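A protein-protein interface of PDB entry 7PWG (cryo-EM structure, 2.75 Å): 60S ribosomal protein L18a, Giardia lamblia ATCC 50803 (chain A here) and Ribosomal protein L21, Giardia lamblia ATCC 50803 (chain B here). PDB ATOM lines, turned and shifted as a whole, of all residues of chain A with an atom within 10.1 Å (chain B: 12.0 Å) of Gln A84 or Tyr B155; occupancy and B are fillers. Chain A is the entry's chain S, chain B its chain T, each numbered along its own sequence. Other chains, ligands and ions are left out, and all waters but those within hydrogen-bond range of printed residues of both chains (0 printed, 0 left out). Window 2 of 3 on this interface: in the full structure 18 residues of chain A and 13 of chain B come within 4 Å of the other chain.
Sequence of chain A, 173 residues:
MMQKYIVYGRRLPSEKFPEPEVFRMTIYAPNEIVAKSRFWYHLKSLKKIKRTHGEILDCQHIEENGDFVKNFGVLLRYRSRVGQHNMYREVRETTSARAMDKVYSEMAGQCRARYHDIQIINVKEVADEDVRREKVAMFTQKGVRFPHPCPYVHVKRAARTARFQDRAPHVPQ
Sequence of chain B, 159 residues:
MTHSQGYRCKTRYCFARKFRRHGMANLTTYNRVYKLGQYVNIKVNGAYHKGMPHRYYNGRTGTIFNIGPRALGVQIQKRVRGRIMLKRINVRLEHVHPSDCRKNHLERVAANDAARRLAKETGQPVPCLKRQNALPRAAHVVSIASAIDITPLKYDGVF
The backbone carbonyl oxygen (O) of Leu B153 sits at hydrogen-bond distance from the guanidinium group (NH1) of Arg A77, at 3.0 Å. ND2 of Asn A86 sits at hydrogen-bond distance from O of Tyr B155, 3.3 Å away.
N of Ile A121 lies within hydrogen-bond range of O of Leu A75, 2.7 Å away. NH2 of Arg A77 is in hydrogen-bond range of OE1 of Gln A84 (2.9 Å). The backbone NH (N) of Gln A119 lies within hydrogen-bond range of the backbone carbonyl oxygen (O) of Arg A77, 2.9 Å away.
Among the printed residues, pairs that only touch across the chains: Ile A120 with Pro B152, Gln A84 with Tyr B155, Leu A46 with Thr B151, Asn A86 with Lys B154, Ile A121 with Pro B152, Arg A77 with Tyr B155, Arg A77 with Lys B154 and Ile A121 with Leu B153.
Of chain B, only Tyr B155 (3.3 Å) comes within 4 Å of Gln A84. Of the printed residues of chain A, Tyr B155 touches Arg A77 (3.7 Å), Gln A84 (3.3 Å) and Asn A86 (3.3 Å). No residue of chain B comes within 4 Å of Tyr A78. No residue of chain B comes within 4 Å of Arg A79. No residue of chain B comes within 4 Å of Ser A80. No residue of chain B comes within 4 Å of His A85. No residue of chain A comes within 4 Å of Asp B156. Printed residues of chain A within 4 Å of Thr B151: Leu A46 (3.4 Å). Printed residues of chain A within 4 Å of Pro B152: Ile A120 and Ile A121. Of the printed residues of chain B, Ile A121 touches Pro B152 (3.6 Å) and Leu B153 (3.9 Å). Of the printed residues of chain B, Leu A46 touches Thr B151. Of the printed residues of chain A, Leu B153 touches Arg A77 (3.0 Å) and Ile A121 (3.9 Å). Ile A118 touches none of the printed residues of chain B.
Hydrophobic or aromatic side chains of chain A that line the printed part of chain B: Leu A46 and Ile A121. Printed residues of chain B that touch a printed residue of chain A: Thr B151, Pro B152, Leu B153, Lys B154 and Tyr B155. Among the printed residues, no Asp or Glu carboxylate lies within 4 Å of a Lys or Arg side-chain nitrogen of the other chain.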
ATOM      1  N   TYR A  41     -42.824  16.247  14.232  1.00  0.00           N
ATOM      2  CA  TYR A  41     -41.927  16.889  13.284  1.00  0.00           C
ATOM      3  C   TYR A  41     -41.009  15.869  12.620  1.00  0.00           C
ATOM      4  O   TYR A  41     -40.668  16.019  11.445  1.00  0.00           O
ATOM      5  CB  TYR A  41     -41.117  17.985  13.976  1.00  0.00           C
ATOM      6  CG  TYR A  41     -39.976  18.530  13.139  1.00  0.00           C
ATOM      7  CD1 TYR A  41     -38.717  17.951  13.180  1.00  0.00           C
ATOM      8  CD2 TYR A  41     -40.157  19.628  12.312  1.00  0.00           C
ATOM      9  CE1 TYR A  41     -37.694  18.434  12.418  1.00  0.00           C
ATOM     10  CE2 TYR A  41     -39.131  20.117  11.558  1.00  0.00           C
ATOM     11  CZ  TYR A  41     -37.902  19.515  11.613  1.00  0.00           C
ATOM     12  OH  TYR A  41     -36.865  20.004  10.862  1.00  0.00           O
ATOM     13  N   SER A  45     -41.129  13.664   8.540  1.00  0.00           N
ATOM     14  CA  SER A  45     -40.005  13.635   7.615  1.00  0.00           C
ATOM     15  C   SER A  45     -39.466  12.225   7.406  1.00  0.00           C
ATOM     16  O   SER A  45     -39.287  11.791   6.271  1.00  0.00           O
ATOM     17  CB  SER A  45     -38.901  14.558   8.124  1.00  0.00           C
ATOM     18  OG  SER A  45     -37.780  14.551   7.260  1.00  0.00           O
ATOM     19  N   LEU A  46     -39.218  11.491   8.485  1.00  0.00           N
ATOM     20  CA  LEU A  46     -38.598  10.176   8.374  1.00  0.00           C
ATOM     21  C   LEU A  46     -39.566   9.114   7.868  1.00  0.00           C
ATOM     22  O   LEU A  46     -39.150   8.173   7.189  1.00  0.00           O
ATOM     23  CB  LEU A  46     -38.032   9.760   9.734  1.00  0.00           C
ATOM     24  CG  LEU A  46     -37.132  10.799  10.410  1.00  0.00           C
ATOM     25  CD1 LEU A  46     -36.837  10.429  11.842  1.00  0.00           C
ATOM     26  CD2 LEU A  46     -35.840  10.972   9.634  1.00  0.00           C
ATOM     27  N   LEU A  75     -24.460  14.159  19.569  1.00  0.00           N
ATOM     28  CA  LEU A  75     -24.317  14.314  18.134  1.00  0.00           C
ATOM     29  C   LEU A  75     -25.558  15.020  17.612  1.00  0.00           C
ATOM     30  O   LEU A  75     -26.668  14.512  17.768  1.00  0.00           O
ATOM     31  CB  LEU A  75     -24.145  12.958  17.462  1.00  0.00           C
ATOM     32  CG  LEU A  75     -23.849  13.069  15.971  1.00  0.00           C
ATOM     33  CD1 LEU A  75     -22.541  13.778  15.786  1.00  0.00           C
ATOM     34  CD2 LEU A  75     -23.826  11.702  15.328  1.00  0.00           C
ATOM     35  N   LEU A  76     -25.382  16.191  17.014  1.00  0.00           N
ATOM     36  CA  LEU A  76     -26.524  16.990  16.602  1.00  0.00           C
ATOM     37  C   LEU A  76     -26.260  17.640  15.253  1.00  0.00           C
ATOM     38  O   LEU A  76     -25.175  17.531  14.682  1.00  0.00           O
ATOM     39  CB  LEU A  76     -26.871  18.049  17.653  1.00  0.00           C
ATOM     40  CG  LEU A  76     -25.784  18.963  18.206  1.00  0.00           C
ATOM     41  CD1 LEU A  76     -25.541  20.148  17.292  1.00  0.00           C
ATOM     42  CD2 LEU A  76     -26.168  19.417  19.591  1.00  0.00           C
ATOM     43  N   ARG A  77     -27.288  18.304  14.740  1.00  0.00           N
ATOM     44  CA  ARG A  77     -27.193  19.123  13.544  1.00  0.00           C
ATOM     45  C   ARG A  77     -27.962  20.412  13.784  1.00  0.00           C
ATOM     46  O   ARG A  77     -28.961  20.428  14.498  1.00  0.00           O
ATOM     47  CB  ARG A  77     -27.720  18.387  12.303  1.00  0.00           C
ATOM     48  CG  ARG A  77     -29.140  17.882  12.399  1.00  0.00           C
ATOM     49  CD  ARG A  77     -29.556  17.106  11.152  1.00  0.00           C
ATOM     50  NE  ARG A  77     -29.964  17.954  10.032  1.00  0.00           N
ATOM     51  CZ  ARG A  77     -30.428  17.492   8.873  1.00  0.00           C
ATOM     52  NH1 ARG A  77     -30.543  16.190   8.672  1.00  0.00           N
ATOM     53  NH2 ARG A  77     -30.785  18.326   7.914  1.00  0.00           N
ATOM     54  N   TYR A  78     -27.485  21.501  13.193  1.00  0.00           N
ATOM     55  CA  TYR A  78     -28.114  22.798  13.379  1.00  0.00           C
ATOM     56  C   TYR A  78     -28.049  23.584  12.081  1.00  0.00           C
ATOM     57  O   TYR A  78     -27.410  23.173  11.116  1.00  0.00           O
ATOM     58  CB  TYR A  78     -27.460  23.580  14.513  1.00  0.00           C
ATOM     59  CG  TYR A  78     -26.097  24.117  14.193  1.00  0.00           C
ATOM     60  CD1 TYR A  78     -25.010  23.275  14.076  1.00  0.00           C
ATOM     61  CD2 TYR A  78     -25.892  25.473  14.037  1.00  0.00           C
ATOM     62  CE1 TYR A  78     -23.769  23.761  13.797  1.00  0.00           C
ATOM     63  CE2 TYR A  78     -24.654  25.972  13.758  1.00  0.00           C
ATOM     64  CZ  TYR A  78     -23.595  25.110  13.642  1.00  0.00           C
ATOM     65  OH  TYR A  78     -22.348  25.603  13.366  1.00  0.00           O
ATOM     66  N   ARG A  79     -28.716  24.731  12.064  1.00  0.00           N
ATOM     67  CA  ARG A  79     -28.801  25.572  10.879  1.00  0.00           C
ATOM     68  C   ARG A  79     -28.263  26.961  11.193  1.00  0.00           C
ATOM     69  O   ARG A  79     -28.623  27.554  12.212  1.00  0.00           O
ATOM     70  CB  ARG A  79     -30.243  25.660  10.374  1.00  0.00           C
ATOM     71  CG  ARG A  79     -30.384  26.366   9.034  1.00  0.00           C
ATOM     72  CD  ARG A  79     -31.831  26.559   8.642  1.00  0.00           C
ATOM     73  NE  ARG A  79     -32.453  25.348   8.121  1.00  0.00           N
ATOM     74  CZ  ARG A  79     -32.497  25.033   6.832  1.00  0.00           C
ATOM     75  NH1 ARG A  79     -31.948  25.833   5.938  1.00  0.00           N
ATOM     76  NH2 ARG A  79     -33.091  23.918   6.436  1.00  0.00           N
ATOM     77  N   SER A  80     -27.395  27.467  10.323  1.00  0.00           N
ATOM     78  CA  SER A  80     -26.874  28.823  10.394  1.00  0.00           C
ATOM     79  C   SER A  80     -27.446  29.623   9.230  1.00  0.00           C
ATOM     80  O   SER A  80     -28.316  29.150   8.501  1.00  0.00           O
ATOM     81  CB  SER A  80     -25.345  28.818  10.376  1.00  0.00           C
ATOM     82  OG  SER A  80     -24.847  28.685   9.055  1.00  0.00           O
ATOM     83  N   ARG A  81     -26.953  30.843   9.048  1.00  0.00           N
ATOM     84  CA  ARG A  81     -27.434  31.663   7.947  1.00  0.00           C
ATOM     85  C   ARG A  81     -26.885  31.245   6.589  1.00  0.00           C
ATOM     86  O   ARG A  81     -27.334  31.786   5.581  1.00  0.00           O
ATOM     87  CB  ARG A  81     -27.120  33.139   8.196  1.00  0.00           C
ATOM     88  CG  ARG A  81     -25.706  33.547   7.897  1.00  0.00           C
ATOM     89  CD  ARG A  81     -25.308  34.739   8.733  1.00  0.00           C
ATOM     90  NE  ARG A  81     -25.452  36.017   8.046  1.00  0.00           N
ATOM     91  CZ  ARG A  81     -24.454  36.638   7.431  1.00  0.00           C
ATOM     92  NH1 ARG A  81     -23.250  36.088   7.406  1.00  0.00           N
ATOM     93  NH2 ARG A  81     -24.655  37.807   6.842  1.00  0.00           N
ATOM     94  N   VAL A  82     -25.947  30.299   6.517  1.00  0.00           N
ATOM     95  CA  VAL A  82     -25.395  29.876   5.237  1.00  0.00           C
ATOM     96  C   VAL A  82     -25.589  28.386   4.973  1.00  0.00           C
ATOM     97  O   VAL A  82     -25.031  27.861   4.015  1.00  0.00           O
ATOM     98  CB  VAL A  82     -23.903  30.250   5.111  1.00  0.00           C
ATOM     99  CG1 VAL A  82     -23.678  31.712   5.428  1.00  0.00           C
ATOM    100  CG2 VAL A  82     -23.038  29.366   5.999  1.00  0.00           C
ATOM    101  N   GLY A  83     -26.348  27.684   5.796  1.00  0.00           N
ATOM    102  CA  GLY A  83     -26.581  26.278   5.530  1.00  0.00           C
ATOM    103  C   GLY A  83     -26.721  25.478   6.809  1.00  0.00           C
ATOM    104  O   GLY A  83     -27.103  26.005   7.842  1.00  0.00           O
ATOM    105  N   GLN A  84     -26.408  24.187   6.703  1.00  0.00           N
ATOM    106  CA  GLN A  84     -26.581  23.229   7.785  1.00  0.00           C
ATOM    107  C   GLN A  84     -25.275  22.499   8.064  1.00  0.00           C
ATOM    108  O   GLN A  84     -24.473  22.263   7.160  1.00  0.00           O
ATOM    109  CB  GLN A  84     -27.683  22.223   7.449  1.00  0.00           C
ATOM    110  CG  GLN A  84     -29.017  22.879   7.212  1.00  0.00           C
ATOM    111  CD  GLN A  84     -30.051  21.926   6.712  1.00  0.00           C
ATOM    112  OE1 GLN A  84     -30.694  21.226   7.488  1.00  0.00           O
ATOM    113  NE2 GLN A  84     -30.219  21.880   5.405  1.00  0.00           N
ATOM    114  N   HIS A  85     -25.077  22.130   9.330  1.00  0.00           N
ATOM    115  CA  HIS A  85     -23.803  21.615   9.812  1.00  0.00           C
ATOM    116  C   HIS A  85     -24.032  20.490  10.812  1.00  0.00           C
ATOM    117  O   HIS A  85     -25.085  20.398  11.439  1.00  0.00           O
ATOM    118  CB  HIS A  85     -22.987  22.738  10.457  1.00  0.00           C
ATOM    119  CG  HIS A  85     -22.942  23.988   9.634  1.00  0.00           C
ATOM    120  ND1 HIS A  85     -22.014  24.186   8.634  1.00  0.00           N
ATOM    121  CD2 HIS A  85     -23.729  25.088   9.638  1.00  0.00           C
ATOM    122  CE1 HIS A  85     -22.221  25.362   8.071  1.00  0.00           C
ATOM    123  NE2 HIS A  85     -23.256  25.929   8.661  1.00  0.00           N
ATOM    124  N   ASN A  86     -23.031  19.629  10.951  1.00  0.00           N
ATOM    125  CA  ASN A  86     -22.996  18.585  11.967  1.00  0.00           C
ATOM    126  C   ASN A  86     -21.981  18.956  13.041  1.00  0.00           C
ATOM    127  O   ASN A  86     -21.020  19.679  12.773  1.00  0.00           O
ATOM    128  CB  ASN A  86     -22.635  17.227  11.360  1.00  0.00           C
ATOM    129  CG  ASN A  86     -23.716  16.678  10.457  1.00  0.00           C
ATOM    130  OD1 ASN A  86     -24.695  16.107  10.924  1.00  0.00           O
ATOM    131  ND2 ASN A  86     -23.533  16.823   9.159  1.00  0.00           N
ATOM    132  N   MET A  87     -22.190  18.462  14.259  1.00  0.00           N
ATOM    133  CA  MET A  87     -21.337  18.842  15.382  1.00  0.00           C
ATOM    134  C   MET A  87     -21.455  17.836  16.513  1.00  0.00           C
ATOM    135  O   MET A  87     -22.552  17.390  16.846  1.00  0.00           O
ATOM    136  CB  MET A  87     -21.687  20.235  15.912  1.00  0.00           C
ATOM    137  N   HIS A 116     -35.574  25.416  18.072  1.00  0.00           N
ATOM    138  CA  HIS A 116     -36.190  24.840  16.884  1.00  0.00           C
ATOM    139  C   HIS A 116     -35.279  24.862  15.664  1.00  0.00           C
ATOM    140  O   HIS A 116     -35.723  24.494  14.580  1.00  0.00           O
ATOM    141  CB  HIS A 116     -37.513  25.542  16.576  1.00  0.00           C
ATOM    142  CG  HIS A 116     -38.644  25.101  17.453  1.00  0.00           C
ATOM    143  ND1 HIS A 116     -39.058  25.817  18.553  1.00  0.00           N
ATOM    144  CD2 HIS A 116     -39.429  24.003  17.407  1.00  0.00           C
ATOM    145  CE1 HIS A 116     -40.053  25.183  19.140  1.00  0.00           C
ATOM    146  NE2 HIS A 116     -40.294  24.077  18.466  1.00  0.00           N
ATOM    147  N   ASP A 117     -34.029  25.284  15.811  1.00  0.00           N
ATOM    148  CA  ASP A 117     -33.039  25.202  14.750  1.00  0.00           C
ATOM    149  C   ASP A 117     -32.176  23.958  14.839  1.00  0.00           C
ATOM    150  O   ASP A 117     -31.319  23.758  13.978  1.00  0.00           O
ATOM    151  CB  ASP A 117     -32.129  26.436  14.770  1.00  0.00           C
ATOM    152  CG  ASP A 117     -32.899  27.721  14.634  1.00  0.00           C
ATOM    153  OD1 ASP A 117     -33.782  27.782  13.753  1.00  0.00           O
ATOM    154  OD2 ASP A 117     -32.631  28.666  15.409  1.00  0.00           O
ATOM    155  N   ILE A 118     -32.397  23.115  15.839  1.00  0.00           N
ATOM    156  CA  ILE A 118     -31.467  22.066  16.231  1.00  0.00           C
ATOM    157  C   ILE A 118     -32.201  20.737  16.208  1.00  0.00           C
ATOM    158  O   ILE A 118     -33.331  20.645  16.698  1.00  0.00           O
ATOM    159  CB  ILE A 118     -30.886  22.347  17.627  1.00  0.00           C
ATOM    160  CG1 ILE A 118     -30.071  23.636  17.611  1.00  0.00           C
ATOM    161  CG2 ILE A 118     -30.072  21.174  18.126  1.00  0.00           C
ATOM    162  CD1 ILE A 118     -29.765  24.180  18.958  1.00  0.00           C
ATOM    163  N   GLN A 119     -31.575  19.717  15.629  1.00  0.00           N
ATOM    164  CA  GLN A 119     -32.064  18.345  15.704  1.00  0.00           C
ATOM    165  C   GLN A 119     -31.005  17.485  16.376  1.00  0.00           C
ATOM    166  O   GLN A 119     -29.850  17.468  15.943  1.00  0.00           O
ATOM    167  CB  GLN A 119     -32.398  17.781  14.318  1.00  0.00           C
ATOM    168  CG  GLN A 119     -33.079  18.759  13.373  1.00  0.00           C
ATOM    169  CD  GLN A 119     -33.444  18.132  12.041  1.00  0.00           C
ATOM    170  OE1 GLN A 119     -33.484  16.915  11.911  1.00  0.00           O
ATOM    171  NE2 GLN A 119     -33.720  18.965  11.048  1.00  0.00           N
ATOM    172  N   ILE A 120     -31.402  16.773  17.423  1.00  0.00           N
ATOM    173  CA  ILE A 120     -30.502  15.912  18.184  1.00  0.00           C
ATOM    174  C   ILE A 120     -30.459  14.543  17.524  1.00  0.00           C
ATOM    175  O   ILE A 120     -31.483  13.868  17.413  1.00  0.00           O
ATOM    176  CB  ILE A 120     -30.956  15.785  19.642  1.00  0.00           C
ATOM    177  CG1 ILE A 120     -31.247  17.159  20.241  1.00  0.00           C
ATOM    178  CG2 ILE A 120     -29.923  15.027  20.437  1.00  0.00           C
ATOM    179  CD1 ILE A 120     -30.087  18.098  20.205  1.00  0.00           C
ATOM    180  N   ILE A 121     -29.274  14.115  17.120  1.00  0.00           N
ATOM    181  CA  ILE A 121     -29.145  12.807  16.503  1.00  0.00           C
ATOM    182  C   ILE A 121     -28.902  11.719  17.545  1.00  0.00           C
ATOM    183  O   ILE A 121     -29.432  10.618  17.425  1.00  0.00           O
ATOM    184  CB  ILE A 121     -28.037  12.853  15.429  1.00  0.00           C
ATOM    185  CG1 ILE A 121     -28.438  13.808  14.312  1.00  0.00           C
ATOM    186  CG2 ILE A 121     -27.774  11.494  14.847  1.00  0.00           C
ATOM    187  CD1 ILE A 121     -27.332  14.655  13.835  1.00  0.00           C
ATOM    188  N   THR B 151     -34.801   7.917  14.763  1.00  0.00           N
ATOM    189  CA  THR B 151     -34.064   9.058  15.280  1.00  0.00           C
ATOM    190  C   THR B 151     -33.749   9.979  14.110  1.00  0.00           C
ATOM    191  O   THR B 151     -33.764   9.538  12.957  1.00  0.00           O
ATOM    192  CB  THR B 151     -32.763   8.614  15.969  1.00  0.00           C
ATOM    193  OG1 THR B 151     -32.305   7.386  15.391  1.00  0.00           O
ATOM    194  CG2 THR B 151     -32.952   8.456  17.480  1.00  0.00           C
ATOM    195  N   PRO B 152     -33.441  11.246  14.370  1.00  0.00           N
ATOM    196  CA  PRO B 152     -33.017  12.137  13.284  1.00  0.00           C
ATOM    197  C   PRO B 152     -31.723  11.668  12.632  1.00  0.00           C
ATOM    198  O   PRO B 152     -30.904  10.983  13.243  1.00  0.00           O
ATOM    199  CB  PRO B 152     -32.822  13.479  13.990  1.00  0.00           C
ATOM    200  CG  PRO B 152     -33.655  13.389  15.188  1.00  0.00           C
ATOM    201  CD  PRO B 152     -33.644  11.980  15.621  1.00  0.00           C
ATOM    202  N   LEU B 153     -31.546  12.045  11.373  1.00  0.00           N
ATOM    203  CA  LEU B 153     -30.393  11.652  10.580  1.00  0.00           C
ATOM    204  C   LEU B 153     -29.432  12.822  10.398  1.00  0.00           C
ATOM    205  O   LEU B 153     -29.774  13.981  10.622  1.00  0.00           O
ATOM    206  CB  LEU B 153     -30.843  11.121   9.221  1.00  0.00           C
ATOM    207  CG  LEU B 153     -31.478   9.737   9.189  1.00  0.00           C
ATOM    208  CD1 LEU B 153     -32.232   9.561   7.901  1.00  0.00           C
ATOM    209  CD2 LEU B 153     -30.414   8.687   9.320  1.00  0.00           C
ATOM    210  N   LYS B 154     -28.216  12.505   9.967  1.00  0.00           N
ATOM    211  CA  LYS B 154     -27.194  13.524   9.778  1.00  0.00           C
ATOM    212  C   LYS B 154     -27.327  14.204   8.422  1.00  0.00           C
ATOM    213  O   LYS B 154     -27.776  13.607   7.442  1.00  0.00           O
ATOM    214  CB  LYS B 154     -25.801  12.923   9.904  1.00  0.00           C
ATOM    215  CG  LYS B 154     -25.481  11.931   8.831  1.00  0.00           C
ATOM    216  CD  LYS B 154     -24.120  11.323   9.022  1.00  0.00           C
ATOM    217  CE  LYS B 154     -23.017  12.330   8.768  1.00  0.00           C
ATOM    218  NZ  LYS B 154     -21.687  11.660   8.782  1.00  0.00           N
ATOM    219  N   TYR B 155     -26.932  15.472   8.377  1.00  0.00           N
ATOM    220  CA  TYR B 155     -26.986  16.234   7.139  1.00  0.00           C
ATOM    221  C   TYR B 155     -25.996  15.677   6.126  1.00  0.00           C
ATOM    222  O   TYR B 155     -24.852  15.366   6.458  1.00  0.00           O
ATOM    223  CB  TYR B 155     -26.694  17.705   7.416  1.00  0.00           C
ATOM    224  CG  TYR B 155     -26.676  18.587   6.193  1.00  0.00           C
ATOM    225  CD1 TYR B 155     -27.849  19.030   5.617  1.00  0.00           C
ATOM    226  CD2 TYR B 155     -25.481  18.981   5.622  1.00  0.00           C
ATOM    227  CE1 TYR B 155     -27.831  19.826   4.507  1.00  0.00           C
ATOM    228  CE2 TYR B 155     -25.449  19.780   4.518  1.00  0.00           C
ATOM    229  CZ  TYR B 155     -26.627  20.204   3.963  1.00  0.00           C
ATOM    230  OH  TYR B 155     -26.597  21.008   2.849  1.00  0.00           O
ATOM    231  N   ASP B 156     -26.446  15.536   4.884  1.00  0.00           N
ATOM    232  CA  ASP B 156     -25.612  15.028   3.800  1.00  0.00           C
ATOM    233  C   ASP B 156     -25.586  16.046   2.668  1.00  0.00           C
ATOM    234  O   ASP B 156     -26.601  16.273   2.003  1.00  0.00           O
ATOM    235  CB  ASP B 156     -26.120  13.685   3.294  1.00  0.00           C
ATOM    236  CG  ASP B 156     -26.129  12.630   4.357  1.00  0.00           C
ATOM    237  OD1 ASP B 156     -25.099  12.462   5.038  1.00  0.00           O
ATOM    238  OD2 ASP B 156     -27.170  11.969   4.516  1.00  0.00           O
ATOM    239  N   GLY B 157     -24.422  16.632   2.432  1.00  0.00           N
ATOM    240  CA  GLY B 157     -24.262  17.612   1.381  1.00  0.00           C
ATOM    241  C   GLY B 157     -22.837  17.656   0.869  1.00  0.00           C
ATOM    242  O   GLY B 157     -21.896  17.805   1.642  1.00  0.00           O
